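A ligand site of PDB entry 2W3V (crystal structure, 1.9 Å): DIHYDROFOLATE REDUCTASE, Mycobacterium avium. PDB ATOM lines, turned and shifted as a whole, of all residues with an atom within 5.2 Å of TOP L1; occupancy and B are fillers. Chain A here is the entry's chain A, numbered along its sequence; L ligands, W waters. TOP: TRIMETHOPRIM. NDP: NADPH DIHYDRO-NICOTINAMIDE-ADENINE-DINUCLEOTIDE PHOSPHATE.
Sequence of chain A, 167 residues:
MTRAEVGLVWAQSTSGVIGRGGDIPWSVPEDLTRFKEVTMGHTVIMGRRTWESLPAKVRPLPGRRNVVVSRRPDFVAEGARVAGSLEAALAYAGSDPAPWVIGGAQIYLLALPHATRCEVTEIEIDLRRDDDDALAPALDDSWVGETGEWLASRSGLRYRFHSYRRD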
ATOM      1  N   VAL A   9      24.524   3.972 -26.330  1.00  0.00           N
ATOM      2  CA  VAL A   9      23.508   2.949 -26.594  1.00  0.00           C
ATOM      3  C   VAL A   9      24.032   1.531 -26.392  1.00  0.00           C
ATOM      4  O   VAL A   9      25.109   1.164 -26.916  1.00  0.00           O
ATOM      5  CB  VAL A   9      22.850   3.152 -28.009  1.00  0.00           C
ATOM      6  CG1 VAL A   9      23.896   3.091 -29.175  1.00  0.00           C
ATOM      7  CG2 VAL A   9      21.681   2.126 -28.216  1.00  0.00           C
ATOM      8  N   TRP A  10      23.279   0.717 -25.660  1.00  0.00           N
ATOM      9  CA  TRP A  10      23.702  -0.675 -25.384  1.00  0.00           C
ATOM     10  C   TRP A  10      22.489  -1.553 -25.021  1.00  0.00           C
ATOM     11  O   TRP A  10      21.417  -1.032 -24.735  1.00  0.00           O
ATOM     12  CB  TRP A  10      24.775  -0.781 -24.277  1.00  0.00           C
ATOM     13  CG  TRP A  10      24.333  -0.574 -22.818  1.00  0.00           C
ATOM     14  CD1 TRP A  10      23.803  -1.519 -21.970  1.00  0.00           C
ATOM     15  CD2 TRP A  10      24.447   0.640 -22.047  1.00  0.00           C
ATOM     16  NE1 TRP A  10      23.574  -0.957 -20.717  1.00  0.00           N
ATOM     17  CE2 TRP A  10      23.948   0.365 -20.751  1.00  0.00           C
ATOM     18  CE3 TRP A  10      24.930   1.929 -22.327  1.00  0.00           C
ATOM     19  CZ2 TRP A  10      23.926   1.318 -19.732  1.00  0.00           C
ATOM     20  CZ3 TRP A  10      24.872   2.924 -21.318  1.00  0.00           C
ATOM     21  CH2 TRP A  10      24.379   2.605 -20.032  1.00  0.00           C
ATOM     22  N   ALA A  11      22.701  -2.862 -25.035  1.00  0.00           N
ATOM     23  CA  ALA A  11      21.723  -3.883 -24.603  1.00  0.00           C
ATOM     24  C   ALA A  11      22.412  -4.684 -23.517  1.00  0.00           C
ATOM     25  O   ALA A  11      23.594  -5.038 -23.693  1.00  0.00           O
ATOM     26  CB  ALA A  11      21.363  -4.813 -25.791  1.00  0.00           C
ATOM     27  N   GLY A  22      33.241 -12.725 -26.737  1.00  0.00           N
ATOM     28  CA  GLY A  22      33.299 -11.806 -27.879  1.00  0.00           C
ATOM     29  C   GLY A  22      31.974 -11.489 -28.559  1.00  0.00           C
ATOM     30  O   GLY A  22      31.930 -10.690 -29.493  1.00  0.00           O
ATOM     31  N   ILE A  24      27.405 -10.988 -28.345  1.00  0.00           N
ATOM     32  CA  ILE A  24      26.205 -10.726 -27.555  1.00  0.00           C
ATOM     33  C   ILE A  24      25.560 -12.095 -27.201  1.00  0.00           C
ATOM     34  O   ILE A  24      25.212 -12.862 -28.107  1.00  0.00           O
ATOM     35  CB  ILE A  24      25.209  -9.814 -28.325  1.00  0.00           C
ATOM     36  CG1 ILE A  24      25.860  -8.453 -28.616  1.00  0.00           C
ATOM     37  CG2 ILE A  24      23.920  -9.649 -27.548  1.00  0.00           C
ATOM     38  CD1 ILE A  24      24.922  -7.363 -29.199  1.00  0.00           C
ATOM     39  N   ASP A  31      15.984  -5.772 -30.564  1.00  0.00           N
ATOM     40  CA  ASP A  31      17.022  -4.840 -30.094  1.00  0.00           C
ATOM     41  C   ASP A  31      17.827  -4.243 -31.278  1.00  0.00           C
ATOM     42  O   ASP A  31      18.172  -3.020 -31.312  1.00  0.00           O
ATOM     43  CB  ASP A  31      17.966  -5.542 -29.095  1.00  0.00           C
ATOM     44  CG  ASP A  31      19.154  -4.690 -28.778  1.00  0.00           C
ATOM     45  OD1 ASP A  31      18.945  -3.610 -28.211  1.00  0.00           O
ATOM     46  OD2 ASP A  31      20.283  -5.085 -29.172  1.00  0.00           O
ATOM     47  N   LEU A  32      18.129  -5.085 -32.273  1.00  0.00           N
ATOM     48  CA  LEU A  32      18.939  -4.601 -33.361  1.00  0.00           C
ATOM     49  C   LEU A  32      18.147  -3.573 -34.161  1.00  0.00           C
ATOM     50  O   LEU A  32      18.721  -2.591 -34.627  1.00  0.00           O
ATOM     51  CB  LEU A  32      19.468  -5.756 -34.219  1.00  0.00           C
ATOM     52  CG  LEU A  32      20.324  -6.716 -33.360  1.00  0.00           C
ATOM     53  CD1 LEU A  32      20.806  -7.839 -34.237  1.00  0.00           C
ATOM     54  CD2 LEU A  32      21.502  -6.025 -32.701  1.00  0.00           C
ATOM     55  N   PHE A  35      18.335  -0.384 -32.213  1.00  0.00           N
ATOM     56  CA  PHE A  35      19.698   0.158 -32.346  1.00  0.00           C
ATOM     57  C   PHE A  35      19.852   0.940 -33.650  1.00  0.00           C
ATOM     58  O   PHE A  35      20.398   2.059 -33.685  1.00  0.00           O
ATOM     59  CB  PHE A  35      20.757  -0.973 -32.273  1.00  0.00           C
ATOM     60  CG  PHE A  35      22.144  -0.540 -32.708  1.00  0.00           C
ATOM     61  CD1 PHE A  35      22.958   0.229 -31.861  1.00  0.00           C
ATOM     62  CD2 PHE A  35      22.644  -0.906 -33.976  1.00  0.00           C
ATOM     63  CE1 PHE A  35      24.251   0.622 -32.290  1.00  0.00           C
ATOM     64  CE2 PHE A  35      23.929  -0.491 -34.400  1.00  0.00           C
ATOM     65  CZ  PHE A  35      24.732   0.267 -33.561  1.00  0.00           C
ATOM     66  N   THR A  50      34.970  -4.180 -30.151  1.00  0.00           N
ATOM     67  CA  THR A  50      33.612  -4.124 -30.672  1.00  0.00           C
ATOM     68  C   THR A  50      33.604  -4.139 -32.215  1.00  0.00           C
ATOM     69  O   THR A  50      32.794  -4.859 -32.838  1.00  0.00           O
ATOM     70  CB  THR A  50      32.862  -2.922 -30.127  1.00  0.00           C
ATOM     71  OG1 THR A  50      32.582  -3.157 -28.731  1.00  0.00           O
ATOM     72  CG2 THR A  50      31.573  -2.775 -30.860  1.00  0.00           C
ATOM     73  N   SER A  53      34.192  -7.600 -33.252  1.00  0.00           N
ATOM     74  CA  SER A  53      33.026  -8.420 -32.931  1.00  0.00           C
ATOM     75  C   SER A  53      31.936  -8.367 -34.007  1.00  0.00           C
ATOM     76  O   SER A  53      31.134  -9.292 -34.144  1.00  0.00           O
ATOM     77  CB  SER A  53      32.407  -8.006 -31.595  1.00  0.00           C
ATOM     78  OG  SER A  53      31.426  -8.963 -31.207  1.00  0.00           O
ATOM     79  N   LEU A  54      31.882  -7.258 -34.754  1.00  0.00           N
ATOM     80  CA  LEU A  54      30.910  -7.124 -35.824  1.00  0.00           C
ATOM     81  C   LEU A  54      31.321  -8.057 -36.949  1.00  0.00           C
ATOM     82  O   LEU A  54      32.494  -8.074 -37.333  1.00  0.00           O
ATOM     83  CB  LEU A  54      30.885  -5.694 -36.353  1.00  0.00           C
ATOM     84  CG  LEU A  54      30.458  -4.592 -35.409  1.00  0.00           C
ATOM     85  CD1 LEU A  54      30.564  -3.253 -36.109  1.00  0.00           C
ATOM     86  CD2 LEU A  54      29.054  -4.809 -34.837  1.00  0.00           C
ATOM     87  N   PRO A  55      30.361  -8.835 -37.481  1.00  0.00           N
ATOM     88  CA  PRO A  55      30.675  -9.648 -38.667  1.00  0.00           C
ATOM     89  C   PRO A  55      31.250  -8.791 -39.802  1.00  0.00           C
ATOM     90  O   PRO A  55      30.781  -7.660 -40.022  1.00  0.00           O
ATOM     91  CB  PRO A  55      29.315 -10.215 -39.072  1.00  0.00           C
ATOM     92  CG  PRO A  55      28.548 -10.253 -37.805  1.00  0.00           C
ATOM     93  CD  PRO A  55      28.966  -9.010 -37.041  1.00  0.00           C
ATOM     94  N   VAL A  58      28.929  -7.253 -42.149  1.00  0.00           N
ATOM     95  CA  VAL A  58      28.015  -6.286 -41.578  1.00  0.00           C
ATOM     96  C   VAL A  58      28.679  -4.925 -41.294  1.00  0.00           C
ATOM     97  O   VAL A  58      27.983  -3.980 -40.917  1.00  0.00           O
ATOM     98  CB  VAL A  58      27.365  -6.884 -40.276  1.00  0.00           C
ATOM     99  CG1 VAL A  58      27.319  -5.895 -39.102  1.00  0.00           C
ATOM    100  CG2 VAL A  58      25.998  -7.478 -40.573  1.00  0.00           C
ATOM    101  N   LEU A  61      28.914  -0.181 -40.311  1.00  0.00           N
ATOM    102  CA  LEU A  61      27.464  -0.070 -40.242  1.00  0.00           C
ATOM    103  C   LEU A  61      26.991   0.939 -41.266  1.00  0.00           C
ATOM    104  O   LEU A  61      27.469   2.093 -41.270  1.00  0.00           O
ATOM    105  CB  LEU A  61      27.042   0.351 -38.831  1.00  0.00           C
ATOM    106  CG  LEU A  61      27.526  -0.633 -37.782  1.00  0.00           C
ATOM    107  CD1 LEU A  61      27.348  -0.069 -36.354  1.00  0.00           C
ATOM    108  CD2 LEU A  61      26.787  -1.961 -37.900  1.00  0.00           C
ATOM    109  N   ILE A 102      28.726   3.226 -29.224  1.00  0.00           N
ATOM    110  CA  ILE A 102      28.014   1.942 -29.413  1.00  0.00           C
ATOM    111  C   ILE A 102      28.749   0.721 -28.818  1.00  0.00           C
ATOM    112  O   ILE A 102      28.395  -0.453 -29.133  1.00  0.00           O
ATOM    113  CB  ILE A 102      27.672   1.702 -30.916  1.00  0.00           C
ATOM    114  CG1 ILE A 102      28.952   1.417 -31.730  1.00  0.00           C
ATOM    115  CG2 ILE A 102      26.877   2.935 -31.485  1.00  0.00           C
ATOM    116  CD1 ILE A 102      28.706   0.767 -33.089  1.00  0.00           C
ATOM    117  N   GLY A 103      29.736   0.970 -27.964  1.00  0.00           N
ATOM    118  CA  GLY A 103      30.404  -0.147 -27.250  1.00  0.00           C
ATOM    119  C   GLY A 103      31.911  -0.165 -27.481  1.00  0.00           C
ATOM    120  O   GLY A 103      32.412   0.592 -28.309  1.00  0.00           O
ATOM    121  N   TYR A 108      32.439   2.604 -23.137  1.00  0.00           N
ATOM    122  CA  TYR A 108      31.355   3.241 -22.365  1.00  0.00           C
ATOM    123  C   TYR A 108      31.889   4.004 -21.155  1.00  0.00           C
ATOM    124  O   TYR A 108      31.443   5.097 -20.874  1.00  0.00           O
ATOM    125  CB  TYR A 108      30.288   2.257 -21.902  1.00  0.00           C
ATOM    126  CG  TYR A 108      29.481   1.631 -23.036  1.00  0.00           C
ATOM    127  CD1 TYR A 108      28.877   2.436 -24.018  1.00  0.00           C
ATOM    128  CD2 TYR A 108      29.277   0.252 -23.088  1.00  0.00           C
ATOM    129  CE1 TYR A 108      28.130   1.850 -25.078  1.00  0.00           C
ATOM    130  CE2 TYR A 108      28.518  -0.335 -24.117  1.00  0.00           C
ATOM    131  CZ  TYR A 108      27.955   0.464 -25.106  1.00  0.00           C
ATOM    132  OH  TYR A 108      27.215  -0.131 -26.113  1.00  0.00           O
ATOM    133  N   THR A 121      18.581  -1.132 -23.870  1.00  0.00           N
ATOM    134  CA  THR A 121      17.593  -2.216 -23.977  1.00  0.00           C
ATOM    135  C   THR A 121      17.890  -3.199 -22.821  1.00  0.00           C
ATOM    136  O   THR A 121      19.027  -3.681 -22.704  1.00  0.00           O
ATOM    137  CB  THR A 121      17.728  -2.970 -25.303  1.00  0.00           C
ATOM    138  OG1 THR A 121      17.573  -2.048 -26.390  1.00  0.00           O
ATOM    139  CG2 THR A 121      16.647  -4.077 -25.418  1.00  0.00           C
HETATM  140  C1  TOP L   1      23.487  -3.488 -30.263  1.00  0.00           C
HETATM  141  N2  TOP L   1      22.331  -3.246 -29.590  1.00  0.00           N
HETATM  142  C3  TOP L   1      22.230  -2.085 -28.834  1.00  0.00           C
HETATM  143  N4  TOP L   1      21.088  -1.818 -28.187  1.00  0.00           N
HETATM  144  N5  TOP L   1      23.256  -1.229 -28.675  1.00  0.00           N
HETATM  145  C6  TOP L   1      24.420  -1.478 -29.326  1.00  0.00           C
HETATM  146  N7  TOP L   1      25.465  -0.637 -29.174  1.00  0.00           N
HETATM  147  C8  TOP L   1      24.569  -2.598 -30.152  1.00  0.00           C
HETATM  148  C9  TOP L   1      25.913  -2.787 -30.871  1.00  0.00           C
HETATM  149  C10 TOP L   1      25.902  -3.949 -31.825  1.00  0.00           C
HETATM  150  C11 TOP L   1      25.126  -4.029 -32.987  1.00  0.00           C
HETATM  151  C12 TOP L   1      25.209  -5.187 -33.785  1.00  0.00           C
HETATM  152  O13 TOP L   1      24.467  -5.329 -34.932  1.00  0.00           O
HETATM  153  C14 TOP L   1      23.876  -4.233 -35.609  1.00  0.00           C
HETATM  154  C15 TOP L   1      26.028  -6.272 -33.422  1.00  0.00           C
HETATM  155  O16 TOP L   1      26.103  -7.407 -34.216  1.00  0.00           O
HETATM  156  C17 TOP L   1      25.145  -8.459 -34.063  1.00  0.00           C
HETATM  157  C18 TOP L   1      26.796  -6.171 -32.266  1.00  0.00           C
HETATM  158  O19 TOP L   1      27.639  -7.193 -31.885  1.00  0.00           O
HETATM  159  C20 TOP L   1      28.679  -6.976 -30.920  1.00  0.00           C
HETATM  160  C21 TOP L   1      26.735  -5.012 -31.498  1.00  0.00           C
HETATM  161  PA  NDP L   2      35.765  -2.304 -26.382  1.00  0.00           P
HETATM  162  O1A NDP L   2      35.435  -1.240 -25.426  1.00  0.00           O
HETATM  163  O2A NDP L   2      34.846  -2.624 -27.536  1.00  0.00           O
HETATM  164  O5B NDP L   2      37.205  -1.935 -26.996  1.00  0.00           O
HETATM  165  C5B NDP L   2      38.357  -1.998 -26.172  1.00  0.00           C
HETATM  166  C4B NDP L   2      39.523  -1.424 -26.962  1.00  0.00           C
HETATM  167  O4B NDP L   2      39.398  -0.002 -27.104  1.00  0.00           O
HETATM  168  C3B NDP L   2      40.878  -1.645 -26.303  1.00  0.00           C
HETATM  169  O3B NDP L   2      41.406  -2.938 -26.568  1.00  0.00           O
HETATM  170  C2B NDP L   2      41.656  -0.535 -26.985  1.00  0.00           C
HETATM  171  O2B NDP L   2      41.971  -0.964 -28.296  1.00  0.00           O
HETATM  172  C1B NDP L   2      40.662   0.612 -27.142  1.00  0.00           C
HETATM  173  N9A NDP L   2      40.789   1.586 -26.051  1.00  0.00           N
HETATM  174  C8A NDP L   2      40.310   1.409 -24.766  1.00  0.00           C
HETATM  175  N7A NDP L   2      40.598   2.510 -24.057  1.00  0.00           N
HETATM  176  C5A NDP L   2      41.250   3.389 -24.867  1.00  0.00           C
HETATM  177  C6A NDP L   2      41.766   4.651 -24.638  1.00  0.00           C
HETATM  178  N6A NDP L   2      41.689   5.210 -23.421  1.00  0.00           N
HETATM  179  N1A NDP L   2      42.370   5.332 -25.672  1.00  0.00           N
HETATM  180  C2A NDP L   2      42.476   4.744 -26.912  1.00  0.00           C
HETATM  181  N3A NDP L   2      41.992   3.499 -27.144  1.00  0.00           N
HETATM  182  C4A NDP L   2      41.359   2.826 -26.133  1.00  0.00           C
HETATM  183  O3  NDP L   2      36.075  -3.712 -25.665  1.00  0.00           O
HETATM  184  PN  NDP L   2      35.274  -4.506 -24.530  1.00  0.00           P
HETATM  185  O1N NDP L   2      35.350  -3.704 -23.311  1.00  0.00           O
HETATM  186  O2N NDP L   2      35.921  -5.848 -24.443  1.00  0.00           O
HETATM  187  O5D NDP L   2      33.778  -4.735 -25.013  1.00  0.00           O
HETATM  188  C5D NDP L   2      33.537  -5.552 -26.141  1.00  0.00           C
HETATM  189  C4D NDP L   2      32.456  -6.553 -25.859  1.00  0.00           C
HETATM  190  O4D NDP L   2      31.202  -5.915 -25.737  1.00  0.00           O
HETATM  191  C3D NDP L   2      32.327  -7.564 -26.983  1.00  0.00           C
HETATM  192  O3D NDP L   2      32.006  -8.825 -26.449  1.00  0.00           O
HETATM  193  C2D NDP L   2      31.076  -7.123 -27.718  1.00  0.00           C
HETATM  194  O2D NDP L   2      30.409  -8.231 -28.303  1.00  0.00           O
HETATM  195  C1D NDP L   2      30.251  -6.538 -26.590  1.00  0.00           C
HETATM  196  N1N NDP L   2      29.269  -5.581 -27.144  1.00  0.00           N
HETATM  197  C2N NDP L   2      27.993  -5.655 -26.662  1.00  0.00           C
HETATM  198  C3N NDP L   2      27.072  -4.659 -26.957  1.00  0.00           C
HETATM  199  C7N NDP L   2      25.710  -4.727 -26.345  1.00  0.00           C
HETATM  200  O7N NDP L   2      24.988  -3.555 -26.448  1.00  0.00           O
HETATM  201  N7N NDP L   2      25.236  -5.838 -25.715  1.00  0.00           N
HETATM  202  C4N NDP L   2      27.454  -3.434 -27.768  1.00  0.00           C
HETATM  203  C5N NDP L   2      28.873  -3.462 -28.275  1.00  0.00           C
HETATM  204  C6N NDP L   2      29.695  -4.533 -27.946  1.00  0.00           C
HETATM  205  P2B NDP L   2      43.485  -1.365 -28.770  1.00  0.00           P
HETATM  206  O1X NDP L   2      43.785  -2.607 -27.957  1.00  0.00           O
HETATM  207  O2X NDP L   2      43.397  -1.760 -30.212  1.00  0.00           O
HETATM  208  O3X NDP L   2      44.383  -0.197 -28.510  1.00  0.00           O
HETATM  209  O   HOH W   1      20.763  -3.145 -36.129  1.00  0.00           O
HETATM  210  O   HOH W   2      22.754  -1.439 -37.287  1.00  0.00           O
HETATM  211  O   HOH W   3      18.930   0.366 -26.616  1.00  0.00           O
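Water W3 lies within hydrogen-bond range of OG1 of Thr 121, O of Trp 10 and N4 of TOP L1.
Residues that only touch TOP L1: Trp 10 (3.4 Å), Phe 35 (3.4 Å), Ser 53 (3.4 Å), Tyr 108 (3.6 Å), Leu 54 (3.6 Å), Ala 11 (3.7 Å), Ile 24 (3.8 Å), Leu 32 (3.8 Å) and Thr 121 (3.95 Å). Hydrophobic or aromatic side chains within 4 Å of TOP L1: Val 9, Ala 11, Ile 24, Leu 32, Phe 35, Leu 54 and Ile 102. The nearest printed residue that does not touch TOP L1 is Pro 55 (4.3 Å).
The side-chain hydroxyl of Tyr 108 sits close to the backbone carbonyl oxygen of Ile 102 (3.3 Å). N of Gly 103 is in hydrogen-bond range of OH of Tyr 108, 3.3 Å away. O of Val 9 is in hydrogen-bond range of OH of Tyr 108 (2.6 Å). The side-chain carboxylate (OD1) of Asp 31 is in hydrogen-bond range of the side-chain hydroxyl (OG1) of Thr 121, 2.8 Å away. N of Thr 121 sits at hydrogen-bond distance from O of Trp 10. OG of Ser 53 sits at hydrogen-bond distance from O of Gly 22.
The side-chain carboxylate (OD2) of Asp 31 lies within hydrogen-bond range of a nitrogen (N2) of TOP L1 (2.8 Å). The backbone carbonyl oxygen of Val 9 is in hydrogen-bond range of a nitrogen (N7) of TOP L1 (2.9 Å). A nitrogen (N7N) of NDP L2 sits at hydrogen-bond distance from the backbone carbonyl oxygen (O) of Ala 11 (2.7 Å). O7N of NDP L2 sits at hydrogen-bond distance from N of Ala 11, 2.8 Å away. OG of Ser 53 is in hydrogen-bond range of O2D of NDP L2 (3.2 Å). The backbone NH (N) of Thr 50 sits at hydrogen-bond distance from an oxygen (O2A) of NDP L2. An oxygen (O2A) of NDP L2 sits at hydrogen-bond distance from the side-chain hydroxyl of Thr 50 (2.6 Å). O2D of NDP L2 is in hydrogen-bond range of O of Gly 22 (3.1 Å). The backbone carbonyl oxygen (O) of Ile 102 sits at hydrogen-bond distance from a nitrogen (N7) of TOP L1.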
